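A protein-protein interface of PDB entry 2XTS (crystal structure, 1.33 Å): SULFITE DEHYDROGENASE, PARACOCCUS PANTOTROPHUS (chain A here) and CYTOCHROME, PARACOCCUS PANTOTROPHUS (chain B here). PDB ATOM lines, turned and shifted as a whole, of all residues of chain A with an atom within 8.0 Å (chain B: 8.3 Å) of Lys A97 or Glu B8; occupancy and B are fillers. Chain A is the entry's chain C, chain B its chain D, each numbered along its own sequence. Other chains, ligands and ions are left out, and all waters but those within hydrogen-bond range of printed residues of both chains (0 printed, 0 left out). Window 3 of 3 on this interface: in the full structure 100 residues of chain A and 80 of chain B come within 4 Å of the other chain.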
ATOM      1  N   ILE A  91      14.897 -19.876 -28.555  1.00  0.00           N
ATOM      2  CA  ILE A  91      16.349 -19.925 -28.460  1.00  0.00           C
ATOM      3  C   ILE A  91      16.702 -19.414 -27.070  1.00  0.00           C
ATOM      4  O   ILE A  91      16.330 -18.295 -26.711  1.00  0.00           O
ATOM      5  CB  ILE A  91      17.052 -19.102 -29.541  1.00  0.00           C
ATOM      6  CG1 ILE A  91      16.567 -19.543 -30.928  1.00  0.00           C
ATOM      7  CG2 ILE A  91      18.568 -19.231 -29.373  1.00  0.00           C
ATOM      8  CD1 ILE A  91      17.353 -18.957 -32.108  1.00  0.00           C
ATOM      9  N   ASN A  92      17.374 -20.228 -26.268  1.00  0.00           N
ATOM     10  CA  ASN A  92      17.706 -19.830 -24.907  1.00  0.00           C
ATOM     11  C   ASN A  92      19.051 -20.400 -24.484  1.00  0.00           C
ATOM     12  O   ASN A  92      19.792 -20.952 -25.297  1.00  0.00           O
ATOM     13  CB  ASN A  92      16.582 -20.237 -23.932  1.00  0.00           C
ATOM     14  CG  ASN A  92      16.608 -21.705 -23.583  1.00  0.00           C
ATOM     15  OD1 ASN A  92      16.476 -22.563 -24.452  1.00  0.00           O
ATOM     16  ND2 ASN A  92      16.754 -21.998 -22.303  1.00  0.00           N
ATOM     17  N   GLY A  93      19.404 -20.177 -23.228  1.00  0.00           N
ATOM     18  CA  GLY A  93      20.665 -20.645 -22.698  1.00  0.00           C
ATOM     19  C   GLY A  93      21.691 -19.542 -22.645  1.00  0.00           C
ATOM     20  O   GLY A  93      21.394 -18.413 -22.231  1.00  0.00           O
ATOM     21  N   LEU A  94      22.892 -19.867 -23.095  1.00  0.00           N
ATOM     22  CA  LEU A  94      24.014 -18.932 -23.111  1.00  0.00           C
ATOM     23  C   LEU A  94      23.934 -18.003 -24.323  1.00  0.00           C
ATOM     24  O   LEU A  94      24.759 -18.036 -25.223  1.00  0.00           O
ATOM     25  CB  LEU A  94      25.332 -19.703 -23.039  1.00  0.00           C
ATOM     26  CG  LEU A  94      25.543 -20.471 -21.729  1.00  0.00           C
ATOM     27  CD1 LEU A  94      26.737 -21.397 -21.848  1.00  0.00           C
ATOM     28  CD2 LEU A  94      25.709 -19.499 -20.562  1.00  0.00           C
ATOM     29  N   VAL A  95      22.891 -17.180 -24.314  1.00  0.00           N
ATOM     30  CA  VAL A  95      22.661 -16.194 -25.352  1.00  0.00           C
ATOM     31  C   VAL A  95      22.428 -14.863 -24.660  1.00  0.00           C
ATOM     32  O   VAL A  95      21.948 -14.813 -23.531  1.00  0.00           O
ATOM     33  CB  VAL A  95      21.469 -16.580 -26.264  1.00  0.00           C
ATOM     34  CG1 VAL A  95      21.786 -17.831 -27.095  1.00  0.00           C
ATOM     35  CG2 VAL A  95      20.193 -16.753 -25.472  1.00  0.00           C
ATOM     36  N   GLU A  96      22.646 -13.770 -25.380  1.00  0.00           N
ATOM     37  CA  GLU A  96      22.471 -12.441 -24.841  1.00  0.00           C
ATOM     38  C   GLU A  96      21.002 -12.123 -24.580  1.00  0.00           C
ATOM     39  O   GLU A  96      20.660 -11.483 -23.589  1.00  0.00           O
ATOM     40  CB  GLU A  96      23.033 -11.397 -25.804  1.00  0.00           C
ATOM     41  CG  GLU A  96      24.027 -10.442 -25.194  1.00  0.00           C
ATOM     42  CD  GLU A  96      25.334 -11.122 -24.832  1.00  0.00           C
ATOM     43  OE1 GLU A  96      25.612 -11.257 -23.624  1.00  0.00           O
ATOM     44  OE2 GLU A  96      26.081 -11.515 -25.754  1.00  0.00           O
ATOM     45  N   LYS A  97      20.117 -12.574 -25.472  1.00  0.00           N
ATOM     46  CA  LYS A  97      18.677 -12.385 -25.319  1.00  0.00           C
ATOM     47  C   LYS A  97      17.974 -13.675 -25.773  1.00  0.00           C
ATOM     48  O   LYS A  97      18.022 -14.022 -26.937  1.00  0.00           O
ATOM     49  CB  LYS A  97      18.193 -11.195 -26.139  1.00  0.00           C
ATOM     50  CG  LYS A  97      16.737 -10.850 -25.890  1.00  0.00           C
ATOM     51  CD  LYS A  97      16.273  -9.700 -26.754  1.00  0.00           C
ATOM     52  CE  LYS A  97      16.797  -8.367 -26.265  1.00  0.00           C
ATOM     53  NZ  LYS A  97      16.182  -7.247 -27.031  1.00  0.00           N
ATOM     54  N   PRO A  98      17.324 -14.352 -24.804  1.00  0.00           N
ATOM     55  CA  PRO A  98      16.551 -15.493 -25.236  1.00  0.00           C
ATOM     56  C   PRO A  98      15.329 -15.024 -26.020  1.00  0.00           C
ATOM     57  O   PRO A  98      14.753 -13.981 -25.686  1.00  0.00           O
ATOM     58  CB  PRO A  98      16.176 -16.169 -23.929  1.00  0.00           C
ATOM     59  CG  PRO A  98      16.102 -15.039 -22.929  1.00  0.00           C
ATOM     60  CD  PRO A  98      17.120 -14.038 -23.373  1.00  0.00           C
ATOM     61  N   LEU A  99      14.970 -15.777 -27.050  1.00  0.00           N
ATOM     62  CA  LEU A  99      13.938 -15.353 -28.003  1.00  0.00           C
ATOM     63  C   LEU A  99      12.875 -16.401 -28.241  1.00  0.00           C
ATOM     64  O   LEU A  99      13.137 -17.598 -28.133  1.00  0.00           O
ATOM     65  CB  LEU A  99      14.574 -15.027 -29.346  1.00  0.00           C
ATOM     66  CG  LEU A  99      15.516 -13.835 -29.354  1.00  0.00           C
ATOM     67  CD1 LEU A  99      16.197 -13.707 -30.686  1.00  0.00           C
ATOM     68  CD2 LEU A  99      14.811 -12.549 -29.004  1.00  0.00           C
ATOM     69  N   VAL A 100      11.678 -15.920 -28.549  1.00  0.00           N
ATOM     70  CA  VAL A 100      10.609 -16.743 -29.071  1.00  0.00           C
ATOM     71  C   VAL A 100      10.274 -16.248 -30.475  1.00  0.00           C
ATOM     72  O   VAL A 100      10.081 -15.052 -30.674  1.00  0.00           O
ATOM     73  CB  VAL A 100       9.357 -16.703 -28.173  1.00  0.00           C
ATOM     74  CG1 VAL A 100       8.211 -17.455 -28.850  1.00  0.00           C
ATOM     75  CG2 VAL A 100       9.658 -17.308 -26.808  1.00  0.00           C
ATOM     76  N   PHE A 101      10.249 -17.170 -31.447  1.00  0.00           N
ATOM     77  CA  PHE A 101       9.807 -16.904 -32.795  1.00  0.00           C
ATOM     78  C   PHE A 101       8.511 -17.609 -33.109  1.00  0.00           C
ATOM     79  O   PHE A 101       8.283 -18.751 -32.703  1.00  0.00           O
ATOM     80  CB  PHE A 101      10.830 -17.414 -33.812  1.00  0.00           C
ATOM     81  CG  PHE A 101      12.189 -16.794 -33.684  1.00  0.00           C
ATOM     82  CD1 PHE A 101      12.437 -15.540 -34.188  1.00  0.00           C
ATOM     83  CD2 PHE A 101      13.225 -17.479 -33.084  1.00  0.00           C
ATOM     84  CE1 PHE A 101      13.688 -14.981 -34.093  1.00  0.00           C
ATOM     85  CE2 PHE A 101      14.480 -16.919 -32.990  1.00  0.00           C
ATOM     86  CZ  PHE A 101      14.711 -15.660 -33.498  1.00  0.00           C
ATOM     87  N   LEU A 156      19.726 -17.385 -37.129  1.00  0.00           N
ATOM     88  CA  LEU A 156      18.824 -17.360 -35.978  1.00  0.00           C
ATOM     89  C   LEU A 156      19.608 -17.115 -34.694  1.00  0.00           C
ATOM     90  O   LEU A 156      19.217 -16.326 -33.826  1.00  0.00           O
ATOM     91  CB  LEU A 156      18.081 -18.686 -35.873  1.00  0.00           C
ATOM     92  CG  LEU A 156      17.210 -19.059 -37.070  1.00  0.00           C
ATOM     93  CD1 LEU A 156      16.552 -20.431 -36.844  1.00  0.00           C
ATOM     94  CD2 LEU A 156      16.162 -17.992 -37.344  1.00  0.00           C
ATOM     95  N   LEU A 157      20.736 -17.804 -34.560  1.00  0.00           N
ATOM     96  CA  LEU A 157      21.545 -17.660 -33.348  1.00  0.00           C
ATOM     97  C   LEU A 157      22.131 -16.259 -33.223  1.00  0.00           C
ATOM     98  O   LEU A 157      22.234 -15.726 -32.122  1.00  0.00           O
ATOM     99  CB  LEU A 157      22.644 -18.717 -33.332  1.00  0.00           C
ATOM    100  CG  LEU A 157      22.083 -20.137 -33.176  1.00  0.00           C
ATOM    101  CD1 LEU A 157      23.184 -21.170 -33.441  1.00  0.00           C
ATOM    102  CD2 LEU A 157      21.400 -20.347 -31.815  1.00  0.00           C
ATOM    103  N   ALA A 158      22.501 -15.658 -34.356  1.00  0.00           N
ATOM    104  CA  ALA A 158      22.983 -14.263 -34.386  1.00  0.00           C
ATOM    105  C   ALA A 158      21.942 -13.308 -33.807  1.00  0.00           C
ATOM    106  O   ALA A 158      22.299 -12.303 -33.171  1.00  0.00           O
ATOM    107  CB  ALA A 158      23.367 -13.846 -35.812  1.00  0.00           C
ATOM    108  N   GLU A 159      20.661 -13.598 -34.016  1.00  0.00           N
ATOM    109  CA  GLU A 159      19.600 -12.756 -33.489  1.00  0.00           C
ATOM    110  C   GLU A 159      19.574 -12.738 -31.951  1.00  0.00           C
ATOM    111  O   GLU A 159      19.378 -11.695 -31.318  1.00  0.00           O
ATOM    112  CB  GLU A 159      18.257 -13.205 -34.061  1.00  0.00           C
ATOM    113  CG  GLU A 159      17.196 -12.149 -34.087  1.00  0.00           C
ATOM    114  CD  GLU A 159      17.477 -10.951 -35.005  1.00  0.00           C
ATOM    115  OE1 GLU A 159      18.276 -11.042 -35.992  1.00  0.00           O
ATOM    116  OE2 GLU A 159      16.838  -9.928 -34.721  1.00  0.00           O
ATOM    117  N   ALA A 160      19.796 -13.908 -31.355  1.00  0.00           N
ATOM    118  CA  ALA A 160      19.834 -14.052 -29.893  1.00  0.00           C
ATOM    119  C   ALA A 160      21.166 -13.585 -29.320  1.00  0.00           C
ATOM    120  O   ALA A 160      21.221 -13.051 -28.227  1.00  0.00           O
ATOM    121  CB  ALA A 160      19.587 -15.507 -29.467  1.00  0.00           C
ATOM    122  N   GLY A 161      22.242 -13.805 -30.059  1.00  0.00           N
ATOM    123  CA  GLY A 161      23.586 -13.404 -29.625  1.00  0.00           C
ATOM    124  C   GLY A 161      24.219 -14.478 -28.763  1.00  0.00           C
ATOM    125  O   GLY A 161      24.044 -14.486 -27.561  1.00  0.00           O
ATOM    126  N   VAL A 162      24.998 -15.362 -29.369  1.00  0.00           N
ATOM    127  CA  VAL A 162      25.616 -16.471 -28.638  1.00  0.00           C
ATOM    128  C   VAL A 162      26.722 -15.926 -27.739  1.00  0.00           C
ATOM    129  O   VAL A 162      27.616 -15.218 -28.192  1.00  0.00           O
ATOM    130  CB  VAL A 162      26.186 -17.532 -29.596  1.00  0.00           C
ATOM    131  CG1 VAL A 162      26.875 -18.647 -28.833  1.00  0.00           C
ATOM    132  CG2 VAL A 162      25.082 -18.123 -30.456  1.00  0.00           C
ATOM    133  N   LYS A 163      26.656 -16.233 -26.448  1.00  0.00           N
ATOM    134  CA  LYS A 163      27.689 -15.807 -25.501  1.00  0.00           C
ATOM    135  C   LYS A 163      29.001 -16.544 -25.730  1.00  0.00           C
ATOM    136  O   LYS A 163      29.020 -17.657 -26.286  1.00  0.00           O
ATOM    137  CB  LYS A 163      27.237 -16.013 -24.063  1.00  0.00           C
ATOM    138  CG  LYS A 163      26.148 -15.080 -23.636  1.00  0.00           C
ATOM    139  CD  LYS A 163      25.752 -15.298 -22.196  1.00  0.00           C
ATOM    140  CE  LYS A 163      24.814 -14.217 -21.743  1.00  0.00           C
ATOM    141  NZ  LYS A 163      24.416 -14.402 -20.335  1.00  0.00           N
ATOM    142  N   LYS B   2      21.701  -7.371 -36.533  1.00  0.00           N
ATOM    143  CA  LYS B   2      20.414  -8.066 -36.205  1.00  0.00           C
ATOM    144  C   LYS B   2      19.231  -7.544 -37.013  1.00  0.00           C
ATOM    145  O   LYS B   2      19.097  -6.352 -37.266  1.00  0.00           O
ATOM    146  CB  LYS B   2      20.073  -7.918 -34.720  1.00  0.00           C
ATOM    147  CG  LYS B   2      21.082  -8.588 -33.815  1.00  0.00           C
ATOM    148  CD  LYS B   2      20.670  -8.582 -32.367  1.00  0.00           C
ATOM    149  CE  LYS B   2      21.769  -9.172 -31.482  1.00  0.00           C
ATOM    150  NZ  LYS B   2      21.390  -9.124 -30.040  1.00  0.00           N
ATOM    151  N   LEU B   5      13.864  -9.536 -35.417  1.00  0.00           N
ATOM    152  CA  LEU B   5      12.797 -10.527 -35.502  1.00  0.00           C
ATOM    153  C   LEU B   5      12.772 -11.336 -34.214  1.00  0.00           C
ATOM    154  O   LEU B   5      13.822 -11.572 -33.597  1.00  0.00           O
ATOM    155  CB  LEU B   5      13.040 -11.469 -36.681  1.00  0.00           C
ATOM    156  CG  LEU B   5      12.882 -10.824 -38.060  1.00  0.00           C
ATOM    157  CD1 LEU B   5      13.400 -11.763 -39.180  1.00  0.00           C
ATOM    158  CD2 LEU B   5      11.419 -10.428 -38.308  1.00  0.00           C
ATOM    159  N   GLY B   6      11.583 -11.777 -33.821  1.00  0.00           N
ATOM    160  CA  GLY B   6      11.394 -12.471 -32.561  1.00  0.00           C
ATOM    161  C   GLY B   6      11.148 -11.502 -31.420  1.00  0.00           C
ATOM    162  O   GLY B   6      11.162 -10.279 -31.600  1.00  0.00           O
ATOM    163  N   ARG B   7      10.855 -12.053 -30.256  1.00  0.00           N
ATOM    164  CA  ARG B   7      10.686 -11.254 -29.049  1.00  0.00           C
ATOM    165  C   ARG B   7      11.304 -11.999 -27.883  1.00  0.00           C
ATOM    166  O   ARG B   7      11.536 -13.206 -27.944  1.00  0.00           O
ATOM    167  CB  ARG B   7       9.210 -10.901 -28.829  1.00  0.00           C
ATOM    168  CG  ARG B   7       8.274 -12.067 -28.788  1.00  0.00           C
ATOM    169  CD  ARG B   7       8.092 -12.570 -27.418  1.00  0.00           C
ATOM    170  NE  ARG B   7       7.143 -13.676 -27.338  1.00  0.00           N
ATOM    171  CZ  ARG B   7       7.037 -14.462 -26.276  1.00  0.00           C
ATOM    172  NH1 ARG B   7       7.822 -14.266 -25.224  1.00  0.00           N
ATOM    173  NH2 ARG B   7       6.168 -15.462 -26.287  1.00  0.00           N
ATOM    174  N   GLU B   8      11.609 -11.263 -26.818  1.00  0.00           N
ATOM    175  CA  GLU B   8      12.280 -11.852 -25.694  1.00  0.00           C
ATOM    176  C   GLU B   8      11.418 -12.899 -25.010  1.00  0.00           C
ATOM    177  O   GLU B   8      10.249 -12.658 -24.687  1.00  0.00           O
ATOM    178  CB  GLU B   8      12.722 -10.796 -24.676  1.00  0.00           C
ATOM    179  CG  GLU B   8      13.524 -11.349 -23.493  1.00  0.00           C
ATOM    180  CD  GLU B   8      14.372 -10.317 -22.776  1.00  0.00           C
ATOM    181  OE1 GLU B   8      14.366  -9.134 -23.174  1.00  0.00           O
ATOM    182  OE2 GLU B   8      15.048 -10.720 -21.810  1.00  0.00           O
ATOM    183  N   ALA B   9      12.020 -14.065 -24.792  1.00  0.00           N
ATOM    184  CA  ALA B   9      11.416 -15.117 -24.011  1.00  0.00           C
ATOM    185  C   ALA B   9      11.310 -14.725 -22.532  1.00  0.00           C
ATOM    186  O   ALA B   9      12.240 -14.159 -21.947  1.00  0.00           O
ATOM    187  CB  ALA B   9      12.190 -16.441 -24.190  1.00  0.00           C
ATOM    188  N   LEU B  10      10.157 -15.022 -21.937  1.00  0.00           N
ATOM    189  CA  LEU B  10       9.924 -14.733 -20.518  1.00  0.00           C
ATOM    190  C   LEU B  10      10.428 -15.862 -19.628  1.00  0.00           C
ATOM    191  O   LEU B  10      10.477 -17.021 -20.056  1.00  0.00           O
ATOM    192  CB  LEU B  10       8.434 -14.484 -20.275  1.00  0.00           C
ATOM    193  CG  LEU B  10       7.852 -13.281 -21.017  1.00  0.00           C
ATOM    194  CD1 LEU B  10       6.377 -13.160 -20.689  1.00  0.00           C
ATOM    195  CD2 LEU B  10       8.631 -12.017 -20.653  1.00  0.00           C
ATOM    196  N   PRO B  11      10.780 -15.541 -18.374  1.00  0.00           N
ATOM    197  CA  PRO B  11      11.240 -16.591 -17.478  1.00  0.00           C
ATOM    198  C   PRO B  11      10.306 -17.809 -17.357  1.00  0.00           C
ATOM    199  O   PRO B  11      10.788 -18.940 -17.330  1.00  0.00           O
ATOM    200  CB  PRO B  11      11.412 -15.852 -16.135  1.00  0.00           C
ATOM    201  CG  PRO B  11      11.626 -14.454 -16.523  1.00  0.00           C
ATOM    202  CD  PRO B  11      10.828 -14.211 -17.728  1.00  0.00           C
ATOM    203  N   GLU B  13       8.298 -18.975 -19.567  1.00  0.00           N
ATOM    204  CA  GLU B  13       8.353 -19.720 -20.828  1.00  0.00           C
ATOM    205  C   GLU B  13       9.612 -20.582 -20.897  1.00  0.00           C
ATOM    206  O   GLU B  13       9.565 -21.767 -21.233  1.00  0.00           O
ATOM    207  CB  GLU B  13       8.308 -18.753 -21.994  1.00  0.00           C
ATOM    208  CG  GLU B  13       6.959 -18.070 -22.139  1.00  0.00           C
ATOM    209  CD  GLU B  13       6.943 -16.897 -23.107  1.00  0.00           C
ATOM    210  OE1 GLU B  13       8.010 -16.267 -23.368  1.00  0.00           O
ATOM    211  OE2 GLU B  13       5.818 -16.573 -23.556  1.00  0.00           O
ATOM    212  N   ILE B  14      10.737 -19.996 -20.532  1.00  0.00           N
ATOM    213  CA  ILE B  14      11.982 -20.746 -20.484  1.00  0.00           C
ATOM    214  C   ILE B  14      11.886 -21.903 -19.493  1.00  0.00           C
ATOM    215  O   ILE B  14      12.291 -23.052 -19.781  1.00  0.00           O
ATOM    216  CB  ILE B  14      13.147 -19.817 -20.102  1.00  0.00           C
ATOM    217  CG1 ILE B  14      13.347 -18.742 -21.198  1.00  0.00           C
ATOM    218  CG2 ILE B  14      14.438 -20.626 -19.849  1.00  0.00           C
ATOM    219  CD1 ILE B  14      14.277 -17.612 -20.806  1.00  0.00           C
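The side-chain carboxylate of Glu A159 lies within hydrogen-bond range of the backbone NH of Leu B5 (3.1 Å).
The backbone NH (N) of Val A100 sits at hydrogen-bond distance from the backbone carbonyl oxygen (O) of Arg B7 (2.8 Å).
The backbone NH of Ala B9 sits at hydrogen-bond distance from the backbone carbonyl oxygen of Pro A98 (2.9 Å).
The backbone NH (N) of Lys A97 sits at hydrogen-bond distance from the backbone carbonyl oxygen (O) of Ala A160.
The backbone NH (N) of Leu B10 sits at hydrogen-bond distance from the side-chain carboxylate (OE1) of Glu B13 (2.9 Å).
O of Ile A91 is in hydrogen-bond range of N of Leu A99 (2.9 Å).
The guanidinium group of Arg B7 lies within salt-bridge range of the side-chain carboxylate of Glu B13, 2.7 Å away.
CG2 of Ile B14 touches ND2 of Asn A92, 3.6 Å away.
Lys A97 touches Glu B8.
O of Pro A98 touches CA of Glu B8, at 3.3 Å.
Pro A98 touches Ile B14.
Arg B7 touches Leu A99 (O to CA, 3.2 Å).
Leu A99 touches Ala B9 (CA to N, 3.96 Å).
Val A100 touches Gly B6 (O to CA, 3.5 Å).
CG2 of Val A100 touches CB of Ala B9, at 3.7 Å.
OE1 of Glu B13 touches CG2 of Val A100, at 3.95 Å.
Phe A101 touches Leu B5.
Of the printed residues of chain B, Asn A92 touches Ile B14 (3.6 Å).
Lys A97 touches one residue of chain B.
Lys A163 touches none of the printed residues of chain B.
Of chain A, only Lys A97 and Pro A98 come within 4 Å of Glu B8.
Of the printed residues of chain A, Glu B13 touches Val A100.
The nearest residue of chain B that does not touch Lys A97 is Lys B2 (5.5 Å).
The nearest printed residue of chain B that does not touch Ala A158 is Leu B5 (8.3 Å).
Of the 10 printed residues of chain B, 8 touch a printed residue of chain A.
Hydrophobic or aromatic side chains of chain B within 4 Å of the printed part of chain A: Ala B9 and Ile B14.
Among the printed residues, no Asp or Glu carboxylate lies within 4 Å of a Lys or Arg side-chain nitrogen of the other chain.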
